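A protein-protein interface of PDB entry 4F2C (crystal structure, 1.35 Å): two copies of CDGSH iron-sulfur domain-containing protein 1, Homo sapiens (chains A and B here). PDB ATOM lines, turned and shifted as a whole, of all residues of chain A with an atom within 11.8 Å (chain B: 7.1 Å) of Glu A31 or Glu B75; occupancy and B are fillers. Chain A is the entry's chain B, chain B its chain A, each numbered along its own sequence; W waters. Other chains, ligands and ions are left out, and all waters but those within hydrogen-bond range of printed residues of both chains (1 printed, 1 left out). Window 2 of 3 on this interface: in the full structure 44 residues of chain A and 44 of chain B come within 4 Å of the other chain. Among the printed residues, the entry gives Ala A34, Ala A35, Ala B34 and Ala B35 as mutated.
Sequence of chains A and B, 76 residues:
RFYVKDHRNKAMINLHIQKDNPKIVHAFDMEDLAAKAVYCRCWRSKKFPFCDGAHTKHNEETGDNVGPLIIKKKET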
ATOM      1  N   ALA A  27      18.563 -13.745  10.350  1.00  0.00           N
ATOM      2  CA  ALA A  27      19.867 -14.325  10.062  1.00  0.00           C
ATOM      3  C   ALA A  27      20.906 -13.219  10.018  1.00  0.00           C
ATOM      4  O   ALA A  27      20.739 -12.213   9.304  1.00  0.00           O
ATOM      5  CB  ALA A  27      19.847 -15.116   8.736  1.00  0.00           C
ATOM      6  N   PHE A  28      21.981 -13.404  10.780  1.00  0.00           N
ATOM      7  CA  PHE A  28      23.066 -12.427  10.852  1.00  0.00           C
ATOM      8  C   PHE A  28      24.414 -13.080  10.628  1.00  0.00           C
ATOM      9  O   PHE A  28      24.611 -14.243  10.977  1.00  0.00           O
ATOM     10  CB  PHE A  28      23.080 -11.757  12.220  1.00  0.00           C
ATOM     11  CG  PHE A  28      21.833 -10.982  12.523  1.00  0.00           C
ATOM     12  CD1 PHE A  28      21.614  -9.747  11.926  1.00  0.00           C
ATOM     13  CD2 PHE A  28      20.866 -11.484  13.378  1.00  0.00           C
ATOM     14  CE1 PHE A  28      20.465  -9.025  12.188  1.00  0.00           C
ATOM     15  CE2 PHE A  28      19.714 -10.764  13.643  1.00  0.00           C
ATOM     16  CZ  PHE A  28      19.515  -9.531  13.049  1.00  0.00           C
ATOM     17  N   ASP A  29      25.344 -12.307  10.072  1.00  0.00           N
ATOM     18  CA  ASP A  29      26.735 -12.722   9.952  1.00  0.00           C
ATOM     19  C   ASP A  29      27.528 -12.087  11.079  1.00  0.00           C
ATOM     20  O   ASP A  29      27.396 -10.900  11.331  1.00  0.00           O
ATOM     21  CB  ASP A  29      27.303 -12.284   8.605  1.00  0.00           C
ATOM     22  CG  ASP A  29      26.597 -12.941   7.440  1.00  0.00           C
ATOM     23  OD1 ASP A  29      26.445 -14.178   7.458  1.00  0.00           O
ATOM     24  OD2 ASP A  29      26.175 -12.217   6.516  1.00  0.00           O
ATOM     25  N   MET A  30      28.346 -12.890  11.756  1.00  0.00           N
ATOM     26  CA  MET A  30      29.084 -12.442  12.936  1.00  0.00           C
ATOM     27  C   MET A  30      29.998 -11.260  12.644  1.00  0.00           C
ATOM     28  O   MET A  30      30.216 -10.406  13.505  1.00  0.00           O
ATOM     29  CB  MET A  30      29.903 -13.594  13.522  1.00  0.00           C
ATOM     30  N   GLU A  31      30.522 -11.204  11.425  1.00  0.00           N
ATOM     31  CA  GLU A  31      31.422 -10.120  11.041  1.00  0.00           C
ATOM     32  C   GLU A  31      30.719  -8.758  11.047  1.00  0.00           C
ATOM     33  O   GLU A  31      31.375  -7.710  11.058  1.00  0.00           O
ATOM     34  CB  GLU A  31      32.051 -10.401   9.671  1.00  0.00           C
ATOM     35  CG  GLU A  31      33.124 -11.498   9.680  1.00  0.00           C
ATOM     36  CD  GLU A  31      32.555 -12.913   9.658  1.00  0.00           C
ATOM     37  OE1 GLU A  31      31.320 -13.081   9.805  1.00  0.00           O
ATOM     38  OE2 GLU A  31      33.354 -13.868   9.485  1.00  0.00           O
ATOM     39  N   ASP A  32      29.388  -8.780  11.056  1.00  0.00           N
ATOM     40  CA  ASP A  32      28.595  -7.554  11.078  1.00  0.00           C
ATOM     41  C   ASP A  32      28.299  -7.082  12.498  1.00  0.00           C
ATOM     42  O   ASP A  32      27.836  -5.959  12.693  1.00  0.00           O
ATOM     43  CB  ASP A  32      27.262  -7.750  10.349  1.00  0.00           C
ATOM     44  CG  ASP A  32      27.420  -7.864   8.846  1.00  0.00           C
ATOM     45  OD1 ASP A  32      28.467  -7.430   8.314  1.00  0.00           O
ATOM     46  OD2 ASP A  32      26.481  -8.381   8.195  1.00  0.00           O
ATOM     47  N   LEU A  33      28.545  -7.942  13.482  1.00  0.00           N
ATOM     48  CA  LEU A  33      28.149  -7.653  14.860  1.00  0.00           C
ATOM     49  C   LEU A  33      29.132  -6.751  15.598  1.00  0.00           C
ATOM     50  O   LEU A  33      30.317  -6.686  15.258  1.00  0.00           O
ATOM     51  CB  LEU A  33      27.951  -8.950  15.655  1.00  0.00           C
ATOM     52  CG  LEU A  33      26.877  -9.905  15.140  1.00  0.00           C
ATOM     53  CD1 LEU A  33      26.612 -11.045  16.124  1.00  0.00           C
ATOM     54  CD2 LEU A  33      25.619  -9.127  14.860  1.00  0.00           C
ATOM     55  N   ALA A  34      28.619  -6.052  16.608  1.00  0.00           N
ATOM     56  CA  ALA A  34      29.460  -5.322  17.549  1.00  0.00           C
ATOM     57  C   ALA A  34      29.968  -6.324  18.577  1.00  0.00           C
ATOM     58  O   ALA A  34      29.568  -7.489  18.553  1.00  0.00           O
ATOM     59  CB  ALA A  34      28.664  -4.215  18.226  1.00  0.00           C
ATOM     60  N   ALA A  35      30.824  -5.872  19.488  1.00  0.00           N
ATOM     61  CA  ALA A  35      31.459  -6.758  20.469  1.00  0.00           C
ATOM     62  C   ALA A  35      30.465  -7.575  21.292  1.00  0.00           C
ATOM     63  O   ALA A  35      30.822  -8.620  21.842  1.00  0.00           O
ATOM     64  CB  ALA A  35      32.379  -5.965  21.395  1.00  0.00           C
ATOM     65  N   LYS A  36      29.228  -7.095  21.380  1.00  0.00           N
ATOM     66  CA  LYS A  36      28.178  -7.829  22.078  1.00  0.00           C
ATOM     67  C   LYS A  36      26.822  -7.594  21.417  1.00  0.00           C
ATOM     68  O   LYS A  36      26.434  -6.451  21.171  1.00  0.00           O
ATOM     69  CB  LYS A  36      28.131  -7.392  23.541  1.00  0.00           C
ATOM     70  CG  LYS A  36      27.113  -8.115  24.393  1.00  0.00           C
ATOM     71  CD  LYS A  36      27.156  -7.593  25.823  1.00  0.00           C
ATOM     72  CE  LYS A  36      26.101  -8.251  26.699  1.00  0.00           C
ATOM     73  NZ  LYS A  36      26.234  -7.861  28.139  1.00  0.00           N
ATOM     74  N   ALA A  37      26.114  -8.680  21.107  1.00  0.00           N
ATOM     75  CA  ALA A  37      24.741  -8.594  20.611  1.00  0.00           C
ATOM     76  C   ALA A  37      23.855  -9.415  21.531  1.00  0.00           C
ATOM     77  O   ALA A  37      24.203 -10.533  21.884  1.00  0.00           O
ATOM     78  CB  ALA A  37      24.640  -9.110  19.171  1.00  0.00           C
ATOM     79  N   TYR A  39      20.185 -10.947  21.871  1.00  0.00           N
ATOM     80  CA  TYR A  39      19.021 -11.292  21.065  1.00  0.00           C
ATOM     81  C   TYR A  39      17.840 -11.733  21.911  1.00  0.00           C
ATOM     82  O   TYR A  39      17.979 -12.524  22.846  1.00  0.00           O
ATOM     83  CB  TYR A  39      19.378 -12.394  20.076  1.00  0.00           C
ATOM     84  CG  TYR A  39      20.399 -11.952  19.063  1.00  0.00           C
ATOM     85  CD1 TYR A  39      20.044 -11.099  18.022  1.00  0.00           C
ATOM     86  CD2 TYR A  39      21.726 -12.380  19.137  1.00  0.00           C
ATOM     87  CE1 TYR A  39      20.975 -10.669  17.096  1.00  0.00           C
ATOM     88  CE2 TYR A  39      22.662 -11.973  18.193  1.00  0.00           C
ATOM     89  CZ  TYR A  39      22.278 -11.118  17.172  1.00  0.00           C
ATOM     90  OH  TYR A  39      23.207 -10.710  16.236  1.00  0.00           O
ATOM     91  N   ILE A  71      25.645 -13.028  21.993  1.00  0.00           N
ATOM     92  CA  ILE A  71      26.837 -13.321  21.216  1.00  0.00           C
ATOM     93  C   ILE A  71      27.856 -12.256  21.559  1.00  0.00           C
ATOM     94  O   ILE A  71      27.594 -11.068  21.405  1.00  0.00           O
ATOM     95  CB  ILE A  71      26.558 -13.301  19.701  1.00  0.00           C
ATOM     96  CG1 ILE A  71      25.477 -14.319  19.343  1.00  0.00           C
ATOM     97  CG2 ILE A  71      27.838 -13.564  18.920  1.00  0.00           C
ATOM     98  CD1 ILE A  71      25.886 -15.774  19.533  1.00  0.00           C
ATOM     99  N   LYS A  72      29.017 -12.664  22.042  1.00  0.00           N
ATOM    100  CA  LYS A  72      29.981 -11.661  22.472  1.00  0.00           C
ATOM    101  C   LYS A  72      31.355 -11.894  21.873  1.00  0.00           C
ATOM    102  O   LYS A  72      31.639 -12.982  21.384  1.00  0.00           O
ATOM    103  CB  LYS A  72      30.044 -11.590  24.004  1.00  0.00           C
ATOM    104  CG  LYS A  72      30.416 -12.895  24.692  1.00  0.00           C
ATOM    105  CD  LYS A  72      29.996 -12.876  26.164  1.00  0.00           C
ATOM    106  CE  LYS A  72      30.299 -14.189  26.868  1.00  0.00           C
ATOM    107  NZ  LYS A  72      31.751 -14.370  27.151  1.00  0.00           N
ATOM    108  N   LYS A  73      32.198 -10.861  21.901  1.00  0.00           N
ATOM    109  CA  LYS A  73      33.607 -11.007  21.531  1.00  0.00           C
ATOM    110  C   LYS A  73      34.388 -11.599  22.703  1.00  0.00           C
ATOM    111  O   LYS A  73      34.088 -11.309  23.867  1.00  0.00           O
ATOM    112  CB  LYS A  73      34.214  -9.661  21.129  1.00  0.00           C
ATOM    113  N   MET B  30      32.072 -15.375  19.927  1.00  0.00           N
ATOM    114  CA  MET B  30      32.123 -15.458  18.466  1.00  0.00           C
ATOM    115  C   MET B  30      33.207 -16.415  17.995  1.00  0.00           C
ATOM    116  O   MET B  30      33.030 -17.155  17.027  1.00  0.00           O
ATOM    117  CB  MET B  30      32.364 -14.076  17.856  1.00  0.00           C
ATOM    118  CG  MET B  30      31.293 -13.060  18.208  1.00  0.00           C
ATOM    119  SD  MET B  30      31.457 -11.458  17.388  1.00  0.00           S
ATOM    120  CE  MET B  30      30.104 -10.573  18.166  1.00  0.00           C
ATOM    121  N   ALA B  34      30.419 -21.950  15.364  1.00  0.00           N
ATOM    122  CA  ALA B  34      30.505 -22.744  14.142  1.00  0.00           C
ATOM    123  C   ALA B  34      30.168 -21.872  12.935  1.00  0.00           C
ATOM    124  O   ALA B  34      29.795 -20.708  13.096  1.00  0.00           O
ATOM    125  CB  ALA B  34      29.553 -23.931  14.214  1.00  0.00           C
ATOM    126  N   ALA B  35      30.295 -22.438  11.737  1.00  0.00           N
ATOM    127  CA  ALA B  35      29.981 -21.700  10.516  1.00  0.00           C
ATOM    128  C   ALA B  35      28.520 -21.253  10.501  1.00  0.00           C
ATOM    129  O   ALA B  35      28.197 -20.197   9.980  1.00  0.00           O
ATOM    130  CB  ALA B  35      30.305 -22.539   9.283  1.00  0.00           C
ATOM    131  N   LYS B  72      25.712 -16.837  11.562  1.00  0.00           N
ATOM    132  CA  LYS B  72      26.688 -17.441  10.670  1.00  0.00           C
ATOM    133  C   LYS B  72      28.003 -16.699  10.753  1.00  0.00           C
ATOM    134  O   LYS B  72      28.058 -15.545  11.203  1.00  0.00           O
ATOM    135  CB  LYS B  72      26.201 -17.379   9.224  1.00  0.00           C
ATOM    136  CG  LYS B  72      24.993 -18.226   8.918  1.00  0.00           C
ATOM    137  CD  LYS B  72      24.439 -17.885   7.542  1.00  0.00           C
ATOM    138  CE  LYS B  72      23.990 -16.424   7.474  1.00  0.00           C
ATOM    139  NZ  LYS B  72      23.487 -16.036   6.121  1.00  0.00           N
ATOM    140  N   LYS B  73      29.058 -17.361  10.297  1.00  0.00           N
ATOM    141  CA  LYS B  73      30.309 -16.673  10.035  1.00  0.00           C
ATOM    142  C   LYS B  73      30.487 -16.547   8.535  1.00  0.00           C
ATOM    143  O   LYS B  73      30.230 -17.497   7.792  1.00  0.00           O
ATOM    144  CB  LYS B  73      31.479 -17.456  10.602  1.00  0.00           C
ATOM    145  CG  LYS B  73      31.417 -17.662  12.094  1.00  0.00           C
ATOM    146  CD  LYS B  73      32.656 -18.400  12.562  1.00  0.00           C
ATOM    147  CE  LYS B  73      32.946 -18.106  14.018  1.00  0.00           C
ATOM    148  NZ  LYS B  73      34.189 -18.766  14.518  1.00  0.00           N
ATOM    149  N   LYS B  74      30.927 -15.378   8.088  1.00  0.00           N
ATOM    150  CA  LYS B  74      31.313 -15.198   6.693  1.00  0.00           C
ATOM    151  C   LYS B  74      32.497 -16.105   6.358  1.00  0.00           C
ATOM    152  O   LYS B  74      32.571 -16.676   5.265  1.00  0.00           O
ATOM    153  CB  LYS B  74      31.685 -13.734   6.420  1.00  0.00           C
ATOM    154  CG  LYS B  74      30.553 -12.738   6.692  1.00  0.00           C
ATOM    155  CD  LYS B  74      30.940 -11.322   6.283  1.00  0.00           C
ATOM    156  CE  LYS B  74      29.803 -10.335   6.535  1.00  0.00           C
ATOM    157  NZ  LYS B  74      28.642 -10.530   5.615  1.00  0.00           N
ATOM    158  N   GLU B  75      33.422 -16.217   7.309  1.00  0.00           N
ATOM    159  CA  GLU B  75      34.600 -17.075   7.196  1.00  0.00           C
ATOM    160  C   GLU B  75      34.854 -17.781   8.518  1.00  0.00           C
ATOM    161  O   GLU B  75      34.710 -17.177   9.580  1.00  0.00           O
ATOM    162  CB  GLU B  75      35.845 -16.247   6.862  1.00  0.00           C
ATOM    163  CG  GLU B  75      35.808 -15.547   5.524  1.00  0.00           C
ATOM    164  CD  GLU B  75      35.968 -16.506   4.341  1.00  0.00           C
ATOM    165  OE1 GLU B  75      36.166 -17.731   4.550  1.00  0.00           O
ATOM    166  OE2 GLU B  75      35.886 -16.024   3.189  1.00  0.00           O
ATOM    167  N   THR B  76      35.252 -19.049   8.460  1.00  0.00           N
ATOM    168  CA  THR B  76      35.570 -19.779   9.687  1.00  0.00           C
ATOM    169  C   THR B  76      36.784 -19.180  10.395  1.00  0.00           C
ATOM    170  O   THR B  76      37.619 -18.509   9.782  1.00  0.00           O
ATOM    171  CB  THR B  76      35.828 -21.268   9.420  1.00  0.00           C
ATOM    172  OG1 THR B  76      36.822 -21.400   8.396  1.00  0.00           O
ATOM    173  CG2 THR B  76      34.541 -21.963   8.983  1.00  0.00           C
ATOM    174  OXT THR B  76      36.943 -19.352  11.608  1.00  0.00           O
HETATM  175  O   HOH W   1      26.906 -15.807   5.540  1.00  0.00           O
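Among the printed residues, merely in contact across the chains: Glu A31 with Lys B73 (3.7 Å), Leu A33 with Met B30 (3.7 Å), Ala A34 with Met B30 (3.2 Å) and Ile A71 with Met B30 (3.6 Å).
Met A30 touches Lys B72, and with the chains exchanged Lys A72 touches Met B30. Ala A34 touches Met B30, but with the chains exchanged Met A30 does not touch Ala B34 (7.1 Å). Of the 12 pairs that touch across the chains among the printed residues, 2 have their exchanged pair printed and touching as well.
The side-chain carboxylate of Asp A29 lies within salt-bridge range of the side-chain amino group of Lys B72, at 3.7 Å. The backbone NH (N) of Glu B75 sits at hydrogen-bond distance from the side-chain carboxylate (OE2) of Glu A31, 3.2 Å away. The backbone NH (N) of Met B30 lies within hydrogen-bond range of the backbone carbonyl oxygen (O) of Lys A72. The backbone NH (N) of Met A30 lies within hydrogen-bond range of the backbone carbonyl oxygen (O) of Lys B72 (2.7 Å). N of Lys B74 sits at hydrogen-bond distance from OE1 of Glu A31, at 2.9 Å. The side-chain amino group of Lys B74 lies within salt-bridge range of the side-chain carboxylate of Asp A32, 3.99 Å away. N of Lys B72 is in hydrogen-bond range of O of Phe A28, at 2.9 Å. The side-chain amino group (NZ) of Lys B74 is in salt-bridge range of the side-chain carboxylate (OD2) of Asp A29 (3.1 Å).
Of the 15 printed residues of chain A, 9 touch a printed residue of chain B. Hydrophobic or aromatic side chains of chain A that line the printed part of chain B: Met A30, Leu A33 and Ile A71. Hydrophobic or aromatic side chains of chain B within 4 Å of the printed part of chain A: Met B30. Among the printed residues, Asp or Glu carboxylates within 4 Å of a Lys or Arg side-chain nitrogen of the other chain: Asp A29 with Lys B72 (3.7 Å), Asp A29 with Lys B74 (3.1 Å) and Asp A32 with Lys B74 (3.99 Å).
Water W1 bridges OD1 of Asp A29 (2.6 Å) and NZ of Lys B72 (3.5 Å).
Printed residues of chain B within 4 Å of Phe A28: Lys B72 (2.9 Å). Of the printed residues of chain B, Asp A29 touches Lys B72 (3.3 Å) and Lys B74 (3.1 Å). Of chain B, only Lys B73, Lys B74 and Glu B75 come within 4 Å of Glu A31. Printed residues of chain B within 4 Å of Leu A33: Met B30 (3.7 Å). No residue of chain A comes within 4 Å of Ala B35. Of chain A, only Glu A31 (3.7 Å) comes within 4 Å of Lys B73. Lys B74 touches just these residues of chain A: Asp A29, Glu A31 and Asp A32. Of chain A, only Glu A31 (3.2 Å) comes within 4 Å of Glu B75. The nearest residue of chain B that does not touch Glu A31 is Lys B72 (4.3 Å). The nearest printed residue of chain B that does not touch Leu A33 is Lys B72 (6.8 Å).
N of Ala A37 is in hydrogen-bond range of O of Ile A71. The backbone NH of Lys B73 lies within hydrogen-bond range of the backbone carbonyl oxygen of Ala B35 (3.0 Å). The backbone carbonyl oxygen (O) of Met B30 sits close to the side-chain amino group (NZ) of Lys B73 (3.2 Å).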
